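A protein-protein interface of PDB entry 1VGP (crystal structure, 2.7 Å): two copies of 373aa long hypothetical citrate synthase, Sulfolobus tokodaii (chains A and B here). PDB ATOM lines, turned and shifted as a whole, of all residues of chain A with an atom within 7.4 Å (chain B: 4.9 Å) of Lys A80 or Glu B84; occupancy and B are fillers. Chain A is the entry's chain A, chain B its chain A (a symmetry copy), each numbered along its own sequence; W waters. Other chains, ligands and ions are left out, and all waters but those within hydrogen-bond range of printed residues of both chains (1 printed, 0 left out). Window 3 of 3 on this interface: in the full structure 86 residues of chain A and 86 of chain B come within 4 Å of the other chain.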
ATOM      1  N   PRO A  75       5.798 -28.619 -15.022  1.00  0.00           N
ATOM      2  CA  PRO A  75       4.916 -29.417 -14.157  1.00  0.00           C
ATOM      3  C   PRO A  75       3.518 -29.560 -14.742  1.00  0.00           C
ATOM      4  O   PRO A  75       3.110 -28.781 -15.607  1.00  0.00           O
ATOM      5  CB  PRO A  75       4.910 -28.648 -12.838  1.00  0.00           C
ATOM      6  CG  PRO A  75       5.262 -27.263 -13.209  1.00  0.00           C
ATOM      7  CD  PRO A  75       6.226 -27.373 -14.359  1.00  0.00           C
ATOM      8  N   ASP A  76       2.783 -30.560 -14.270  1.00  0.00           N
ATOM      9  CA  ASP A  76       1.513 -30.926 -14.890  1.00  0.00           C
ATOM     10  C   ASP A  76       0.490 -29.799 -14.830  1.00  0.00           C
ATOM     11  O   ASP A  76      -0.311 -29.624 -15.757  1.00  0.00           O
ATOM     12  CB  ASP A  76       0.935 -32.168 -14.219  1.00  0.00           C
ATOM     13  CG  ASP A  76       1.966 -33.250 -14.027  1.00  0.00           C
ATOM     14  OD1 ASP A  76       2.797 -33.103 -13.103  1.00  0.00           O
ATOM     15  OD2 ASP A  76       1.951 -34.234 -14.800  1.00  0.00           O
ATOM     16  N   PHE A  77       0.511 -29.049 -13.733  1.00  0.00           N
ATOM     17  CA  PHE A  77      -0.455 -27.989 -13.544  1.00  0.00           C
ATOM     18  C   PHE A  77      -0.351 -26.980 -14.680  1.00  0.00           C
ATOM     19  O   PHE A  77      -1.356 -26.638 -15.303  1.00  0.00           O
ATOM     20  CB  PHE A  77      -0.241 -27.293 -12.192  1.00  0.00           C
ATOM     21  CG  PHE A  77      -1.395 -26.427 -11.764  1.00  0.00           C
ATOM     22  CD1 PHE A  77      -2.701 -26.906 -11.824  1.00  0.00           C
ATOM     23  CD2 PHE A  77      -1.178 -25.132 -11.312  1.00  0.00           C
ATOM     24  CE1 PHE A  77      -3.780 -26.103 -11.441  1.00  0.00           C
ATOM     25  CE2 PHE A  77      -2.246 -24.322 -10.927  1.00  0.00           C
ATOM     26  CZ  PHE A  77      -3.553 -24.807 -10.991  1.00  0.00           C
ATOM     27  N   ILE A  78       0.861 -26.517 -14.974  1.00  0.00           N
ATOM     28  CA  ILE A  78       1.012 -25.508 -16.017  1.00  0.00           C
ATOM     29  C   ILE A  78       0.777 -26.094 -17.419  1.00  0.00           C
ATOM     30  O   ILE A  78       0.232 -25.421 -18.303  1.00  0.00           O
ATOM     31  CB  ILE A  78       2.414 -24.767 -15.939  1.00  0.00           C
ATOM     32  CG1 ILE A  78       3.450 -25.506 -16.775  1.00  0.00           C
ATOM     33  CG2 ILE A  78       2.895 -24.646 -14.489  1.00  0.00           C
ATOM     34  CD1 ILE A  78       3.793 -24.780 -18.065  1.00  0.00           C
ATOM     35  N   ILE A  79       1.147 -27.356 -17.620  1.00  0.00           N
ATOM     36  CA  ILE A  79       0.791 -28.040 -18.870  1.00  0.00           C
ATOM     37  C   ILE A  79      -0.727 -28.155 -19.017  1.00  0.00           C
ATOM     38  O   ILE A  79      -1.276 -28.004 -20.113  1.00  0.00           O
ATOM     39  CB  ILE A  79       1.432 -29.446 -18.936  1.00  0.00           C
ATOM     40  CG1 ILE A  79       2.877 -29.316 -19.427  1.00  0.00           C
ATOM     41  CG2 ILE A  79       0.657 -30.340 -19.887  1.00  0.00           C
ATOM     42  CD1 ILE A  79       3.721 -30.543 -19.216  1.00  0.00           C
ATOM     43  N   LYS A  80      -1.397 -28.410 -17.898  1.00  0.00           N
ATOM     44  CA  LYS A  80      -2.855 -28.433 -17.840  1.00  0.00           C
ATOM     45  C   LYS A  80      -3.407 -27.067 -18.227  1.00  0.00           C
ATOM     46  O   LYS A  80      -4.379 -26.948 -18.981  1.00  0.00           O
ATOM     47  CB  LYS A  80      -3.281 -28.790 -16.416  1.00  0.00           C
ATOM     48  CG  LYS A  80      -4.759 -29.008 -16.208  1.00  0.00           C
ATOM     49  CD  LYS A  80      -4.962 -29.846 -14.955  1.00  0.00           C
ATOM     50  CE  LYS A  80      -6.379 -29.729 -14.388  1.00  0.00           C
ATOM     51  NZ  LYS A  80      -7.436 -30.193 -15.334  1.00  0.00           N
ATOM     52  N   PHE A  81      -2.763 -26.036 -17.690  1.00  0.00           N
ATOM     53  CA  PHE A  81      -3.072 -24.660 -18.039  1.00  0.00           C
ATOM     54  C   PHE A  81      -3.020 -24.463 -19.548  1.00  0.00           C
ATOM     55  O   PHE A  81      -3.928 -23.877 -20.138  1.00  0.00           O
ATOM     56  CB  PHE A  81      -2.071 -23.716 -17.360  1.00  0.00           C
ATOM     57  CG  PHE A  81      -2.066 -22.325 -17.931  1.00  0.00           C
ATOM     58  CD1 PHE A  81      -3.209 -21.525 -17.876  1.00  0.00           C
ATOM     59  CD2 PHE A  81      -0.910 -21.809 -18.517  1.00  0.00           C
ATOM     60  CE1 PHE A  81      -3.203 -20.234 -18.395  1.00  0.00           C
ATOM     61  CE2 PHE A  81      -0.894 -20.522 -19.036  1.00  0.00           C
ATOM     62  CZ  PHE A  81      -2.045 -19.730 -18.976  1.00  0.00           C
ATOM     63  N   LEU A  82      -1.946 -24.950 -20.164  1.00  0.00           N
ATOM     64  CA  LEU A  82      -1.692 -24.650 -21.560  1.00  0.00           C
ATOM     65  C   LEU A  82      -2.788 -25.228 -22.451  1.00  0.00           C
ATOM     66  O   LEU A  82      -3.369 -24.516 -23.282  1.00  0.00           O
ATOM     67  CB  LEU A  82      -0.323 -25.185 -21.981  1.00  0.00           C
ATOM     68  CG  LEU A  82       0.873 -24.453 -21.353  1.00  0.00           C
ATOM     69  CD1 LEU A  82       2.171 -25.071 -21.833  1.00  0.00           C
ATOM     70  CD2 LEU A  82       0.830 -22.979 -21.723  1.00  0.00           C
ATOM     71  N   ARG A  83      -3.092 -26.512 -22.269  1.00  0.00           N
ATOM     72  CA  ARG A  83      -4.073 -27.150 -23.138  1.00  0.00           C
ATOM     73  C   ARG A  83      -5.511 -26.796 -22.778  1.00  0.00           C
ATOM     74  O   ARG A  83      -6.415 -26.948 -23.599  1.00  0.00           O
ATOM     75  CB  ARG A  83      -3.906 -28.673 -23.153  1.00  0.00           C
ATOM     76  CG  ARG A  83      -3.302 -29.291 -21.920  1.00  0.00           C
ATOM     77  CD  ARG A  83      -3.559 -30.794 -21.930  1.00  0.00           C
ATOM     78  NE  ARG A  83      -2.341 -31.601 -21.954  1.00  0.00           N
ATOM     79  CZ  ARG A  83      -1.906 -32.275 -23.018  1.00  0.00           C
ATOM     80  NH1 ARG A  83      -2.498 -32.128 -24.200  1.00  0.00           N
ATOM     81  NH2 ARG A  83      -0.881 -33.111 -22.900  1.00  0.00           N
ATOM     82  N   GLU A  84      -5.719 -26.307 -21.562  1.00  0.00           N
ATOM     83  CA  GLU A  84      -7.057 -25.936 -21.135  1.00  0.00           C
ATOM     84  C   GLU A  84      -7.409 -24.502 -21.517  1.00  0.00           C
ATOM     85  O   GLU A  84      -8.582 -24.159 -21.629  1.00  0.00           O
ATOM     86  CB  GLU A  84      -7.200 -26.121 -19.626  1.00  0.00           C
ATOM     87  CG  GLU A  84      -7.682 -27.506 -19.216  1.00  0.00           C
ATOM     88  CD  GLU A  84      -8.475 -27.497 -17.920  1.00  0.00           C
ATOM     89  OE1 GLU A  84      -9.431 -26.682 -17.811  1.00  0.00           O
ATOM     90  OE2 GLU A  84      -8.151 -28.296 -17.009  1.00  0.00           O
ATOM     91  N   VAL A  85      -6.389 -23.678 -21.731  1.00  0.00           N
ATOM     92  CA  VAL A  85      -6.574 -22.239 -21.877  1.00  0.00           C
ATOM     93  C   VAL A  85      -7.174 -21.803 -23.224  1.00  0.00           C
ATOM     94  O   VAL A  85      -7.008 -22.470 -24.250  1.00  0.00           O
ATOM     95  CB  VAL A  85      -5.224 -21.493 -21.656  1.00  0.00           C
ATOM     96  CG1 VAL A  85      -4.295 -21.694 -22.860  1.00  0.00           C
ATOM     97  CG2 VAL A  85      -5.481 -20.018 -21.401  1.00  0.00           C
ATOM     98  N   LYS A  87      -7.436 -20.472 -26.647  1.00  0.00           N
ATOM     99  CA  LYS A  87      -6.404 -20.683 -27.658  1.00  0.00           C
ATOM    100  C   LYS A  87      -6.253 -19.499 -28.602  1.00  0.00           C
ATOM    101  O   LYS A  87      -5.466 -19.549 -29.546  1.00  0.00           O
ATOM    102  CB  LYS A  87      -6.693 -21.952 -28.456  1.00  0.00           C
ATOM    103  CG  LYS A  87      -6.512 -23.227 -27.643  1.00  0.00           C
ATOM    104  CD  LYS A  87      -5.049 -23.477 -27.300  1.00  0.00           C
ATOM    105  CE  LYS A  87      -4.876 -24.695 -26.391  1.00  0.00           C
ATOM    106  NZ  LYS A  87      -5.355 -24.456 -25.005  1.00  0.00           N
ATOM    107  N   GLU A 105       4.566 -23.363  -8.245  1.00  0.00           N
ATOM    108  CA  GLU A 105       4.943 -24.771  -8.174  1.00  0.00           C
ATOM    109  C   GLU A 105       6.346 -24.986  -7.620  1.00  0.00           C
ATOM    110  O   GLU A 105       6.710 -26.107  -7.273  1.00  0.00           O
ATOM    111  CB  GLU A 105       4.821 -25.419  -9.552  1.00  0.00           C
ATOM    112  CG  GLU A 105       3.382 -25.585 -10.014  1.00  0.00           C
ATOM    113  CD  GLU A 105       2.525 -26.315  -8.990  1.00  0.00           C
ATOM    114  OE1 GLU A 105       1.333 -25.967  -8.843  1.00  0.00           O
ATOM    115  OE2 GLU A 105       3.046 -27.239  -8.327  1.00  0.00           O
ATOM    116  N   LEU A 134      -0.361 -26.911 -29.289  1.00  0.00           N
ATOM    117  CA  LEU A 134      -1.710 -26.925 -28.731  1.00  0.00           C
ATOM    118  C   LEU A 134      -2.625 -25.951 -29.466  1.00  0.00           C
ATOM    119  O   LEU A 134      -3.783 -26.249 -29.733  1.00  0.00           O
ATOM    120  CB  LEU A 134      -1.653 -26.558 -27.249  1.00  0.00           C
ATOM    121  CG  LEU A 134      -1.637 -27.696 -26.230  1.00  0.00           C
ATOM    122  CD1 LEU A 134      -1.099 -28.970 -26.854  1.00  0.00           C
ATOM    123  CD2 LEU A 134      -0.788 -27.275 -25.038  1.00  0.00           C
ATOM    124  N   ILE A 140       1.296 -31.621 -27.357  1.00  0.00           N
ATOM    125  CA  ILE A 140       2.568 -31.433 -26.687  1.00  0.00           C
ATOM    126  C   ILE A 140       3.514 -32.542 -27.114  1.00  0.00           C
ATOM    127  O   ILE A 140       3.199 -33.723 -27.016  1.00  0.00           O
ATOM    128  CB  ILE A 140       2.407 -31.469 -25.158  1.00  0.00           C
ATOM    129  CG1 ILE A 140       1.516 -30.308 -24.727  1.00  0.00           C
ATOM    130  CG2 ILE A 140       3.771 -31.376 -24.474  1.00  0.00           C
ATOM    131  CD1 ILE A 140       1.183 -30.319 -23.257  1.00  0.00           C
ATOM    132  N   LYS B  80     -11.576 -21.962 -11.286  1.00  0.00           N
ATOM    133  CA  LYS B  80     -11.051 -23.315 -11.439  1.00  0.00           C
ATOM    134  C   LYS B  80      -9.605 -23.363 -10.962  1.00  0.00           C
ATOM    135  O   LYS B  80      -9.181 -24.290 -10.263  1.00  0.00           O
ATOM    136  CB  LYS B  80     -11.132 -23.707 -12.914  1.00  0.00           C
ATOM    137  CG  LYS B  80     -10.771 -25.136 -13.235  1.00  0.00           C
ATOM    138  CD  LYS B  80     -11.392 -25.513 -14.571  1.00  0.00           C
ATOM    139  CE  LYS B  80     -10.721 -26.729 -15.214  1.00  0.00           C
ATOM    140  NZ  LYS B  80     -10.816 -27.966 -14.384  1.00  0.00           N
ATOM    141  N   PHE B  81      -8.856 -22.340 -11.357  1.00  0.00           N
ATOM    142  CA  PHE B  81      -7.489 -22.155 -10.901  1.00  0.00           C
ATOM    143  C   PHE B  81      -7.422 -22.176  -9.380  1.00  0.00           C
ATOM    144  O   PHE B  81      -6.579 -22.858  -8.797  1.00  0.00           O
ATOM    145  CB  PHE B  81      -6.944 -20.819 -11.423  1.00  0.00           C
ATOM    146  CG  PHE B  81      -5.694 -20.359 -10.726  1.00  0.00           C
ATOM    147  CD1 PHE B  81      -4.525 -21.120 -10.778  1.00  0.00           C
ATOM    148  CD2 PHE B  81      -5.684 -19.155 -10.021  1.00  0.00           C
ATOM    149  CE1 PHE B  81      -3.364 -20.691 -10.141  1.00  0.00           C
ATOM    150  CE2 PHE B  81      -4.532 -18.718  -9.385  1.00  0.00           C
ATOM    151  CZ  PHE B  81      -3.365 -19.489  -9.443  1.00  0.00           C
ATOM    152  N   LEU B  82      -8.312 -21.418  -8.746  1.00  0.00           N
ATOM    153  CA  LEU B  82      -8.217 -21.203  -7.314  1.00  0.00           C
ATOM    154  C   LEU B  82      -8.401 -22.513  -6.553  1.00  0.00           C
ATOM    155  O   LEU B  82      -7.579 -22.869  -5.697  1.00  0.00           O
ATOM    156  CB  LEU B  82      -9.249 -20.170  -6.859  1.00  0.00           C
ATOM    157  CG  LEU B  82      -8.976 -18.737  -7.338  1.00  0.00           C
ATOM    158  CD1 LEU B  82     -10.061 -17.806  -6.837  1.00  0.00           C
ATOM    159  CD2 LEU B  82      -7.619 -18.272  -6.836  1.00  0.00           C
ATOM    160  N   ARG B  83      -9.465 -23.248  -6.874  1.00  0.00           N
ATOM    161  CA  ARG B  83      -9.746 -24.470  -6.132  1.00  0.00           C
ATOM    162  C   ARG B  83      -8.860 -25.639  -6.547  1.00  0.00           C
ATOM    163  O   ARG B  83      -8.717 -26.609  -5.804  1.00  0.00           O
ATOM    164  CB  ARG B  83     -11.220 -24.874  -6.249  1.00  0.00           C
ATOM    165  CG  ARG B  83     -11.939 -24.426  -7.494  1.00  0.00           C
ATOM    166  CD  ARG B  83     -13.235 -25.214  -7.641  1.00  0.00           C
ATOM    167  NE  ARG B  83     -14.437 -24.384  -7.616  1.00  0.00           N
ATOM    168  CZ  ARG B  83     -15.291 -24.327  -6.594  1.00  0.00           C
ATOM    169  NH1 ARG B  83     -15.009 -24.932  -5.443  1.00  0.00           N
ATOM    170  NH2 ARG B  83     -16.439 -23.672  -6.725  1.00  0.00           N
ATOM    171  N   GLU B  84      -8.253 -25.538  -7.723  1.00  0.00           N
ATOM    172  CA  GLU B  84      -7.384 -26.602  -8.197  1.00  0.00           C
ATOM    173  C   GLU B  84      -5.949 -26.439  -7.706  1.00  0.00           C
ATOM    174  O   GLU B  84      -5.203 -27.411  -7.637  1.00  0.00           O
ATOM    175  CB  GLU B  84      -7.406 -26.661  -9.724  1.00  0.00           C
ATOM    176  CG  GLU B  84      -8.484 -27.575 -10.291  1.00  0.00           C
ATOM    177  CD  GLU B  84      -8.098 -28.185 -11.628  1.00  0.00           C
ATOM    178  OE1 GLU B  84      -6.980 -28.761 -11.721  1.00  0.00           O
ATOM    179  OE2 GLU B  84      -8.901 -28.092 -12.588  1.00  0.00           O
ATOM    180  N   VAL B  85      -5.580 -25.214  -7.352  1.00  0.00           N
ATOM    181  CA  VAL B  85      -4.188 -24.872  -7.083  1.00  0.00           C
ATOM    182  C   VAL B  85      -3.646 -25.395  -5.742  1.00  0.00           C
ATOM    183  O   VAL B  85      -4.391 -25.581  -4.775  1.00  0.00           O
ATOM    184  CB  VAL B  85      -3.985 -23.328  -7.147  1.00  0.00           C
ATOM    185  CG1 VAL B  85      -4.594 -22.654  -5.911  1.00  0.00           C
ATOM    186  CG2 VAL B  85      -2.508 -23.003  -7.279  1.00  0.00           C
ATOM    187  N   ARG B  86      -2.341 -25.644  -5.707  1.00  0.00           N
ATOM    188  CA  ARG B  86      -1.600 -25.802  -4.461  1.00  0.00           C
ATOM    189  C   ARG B  86      -2.203 -24.902  -3.388  1.00  0.00           C
ATOM    190  O   ARG B  86      -2.379 -23.703  -3.601  1.00  0.00           O
ATOM    191  CB  ARG B  86      -0.139 -25.426  -4.702  1.00  0.00           C
ATOM    192  CG  ARG B  86       0.785 -25.686  -3.540  1.00  0.00           C
ATOM    193  CD  ARG B  86       2.203 -25.299  -3.913  1.00  0.00           C
ATOM    194  NE  ARG B  86       3.207 -26.067  -3.175  1.00  0.00           N
ATOM    195  CZ  ARG B  86       4.245 -26.668  -3.746  1.00  0.00           C
ATOM    196  NH1 ARG B  86       5.135 -27.302  -3.002  1.00  0.00           N
ATOM    197  NH2 ARG B  86       4.387 -26.637  -5.065  1.00  0.00           N
ATOM    198  N   LYS B  87      -2.534 -25.471  -2.233  1.00  0.00           N
ATOM    199  CA  LYS B  87      -3.177 -24.688  -1.183  1.00  0.00           C
ATOM    200  C   LYS B  87      -2.197 -24.203  -0.124  1.00  0.00           C
ATOM    201  O   LYS B  87      -2.597 -23.581   0.859  1.00  0.00           O
ATOM    202  CB  LYS B  87      -4.296 -25.494  -0.528  1.00  0.00           C
ATOM    203  CG  LYS B  87      -5.493 -25.717  -1.443  1.00  0.00           C
ATOM    204  CD  LYS B  87      -6.247 -24.421  -1.714  1.00  0.00           C
ATOM    205  CE  LYS B  87      -7.381 -24.622  -2.721  1.00  0.00           C
ATOM    206  NZ  LYS B  87      -6.893 -24.848  -4.106  1.00  0.00           N
HETATM  207  O   HOH W   1      -1.085 -27.307  -8.032  1.00  0.00           O
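The side-chain carboxylate (OE2) of Glu B84 is in salt-bridge range of the side-chain amino group (NZ) of Lys A80 (3.8 Å). The side-chain amino group of Lys B80 is in salt-bridge range of the side-chain carboxylate of Glu A84 (3.8 Å). The side-chain carboxylate (OE2) of Glu A105 is in salt-bridge range of the guanidinium group (NH2) of Arg B86 (3.6 Å).
NZ of Lys A80 lies within salt-bridge range of OE2 of Glu A84, at 2.6 Å. The side-chain carboxylate (OE2) of Glu B84 is in salt-bridge range of the side-chain amino group (NZ) of Lys B80 (2.6 Å). The backbone carbonyl oxygen (O) of Val B85 lies within hydrogen-bond range of the side-chain amino group (NZ) of Lys B87 (2.7 Å).
Phe A77 touches Phe B81. CE2 of Phe A77 touches CG2 of Val B85 (3.9 Å).
Of chain A, only Lys A80 (2.9 Å) comes within 4 Å of Glu B84. Of the printed residues of chain A, Arg B86 touches Glu A105 (3.2 Å). Of the printed residues of chain B, Phe A77 touches Phe B81 and Val B85. Printed residues of chain A within 4 Å of Val B85: Phe A77 (3.9 Å). Lys A87 touches none of the printed residues of chain B. The nearest residue of chain B that does not touch Lys A80 is Lys B80 (4.2 Å).
Hydrophobic or aromatic side chains of chain B within 4 Å of the printed part of chain A: Phe B81 and Val B85. Among the printed residues, 5 pairs touch across the chains.
Lys A80 touches Glu B84, and with the chains exchanged Glu A84 touches Lys B80.
Water W1 lies within hydrogen-bond range of the side-chain carboxylate of Glu A105 and the backbone NH of Arg B86.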
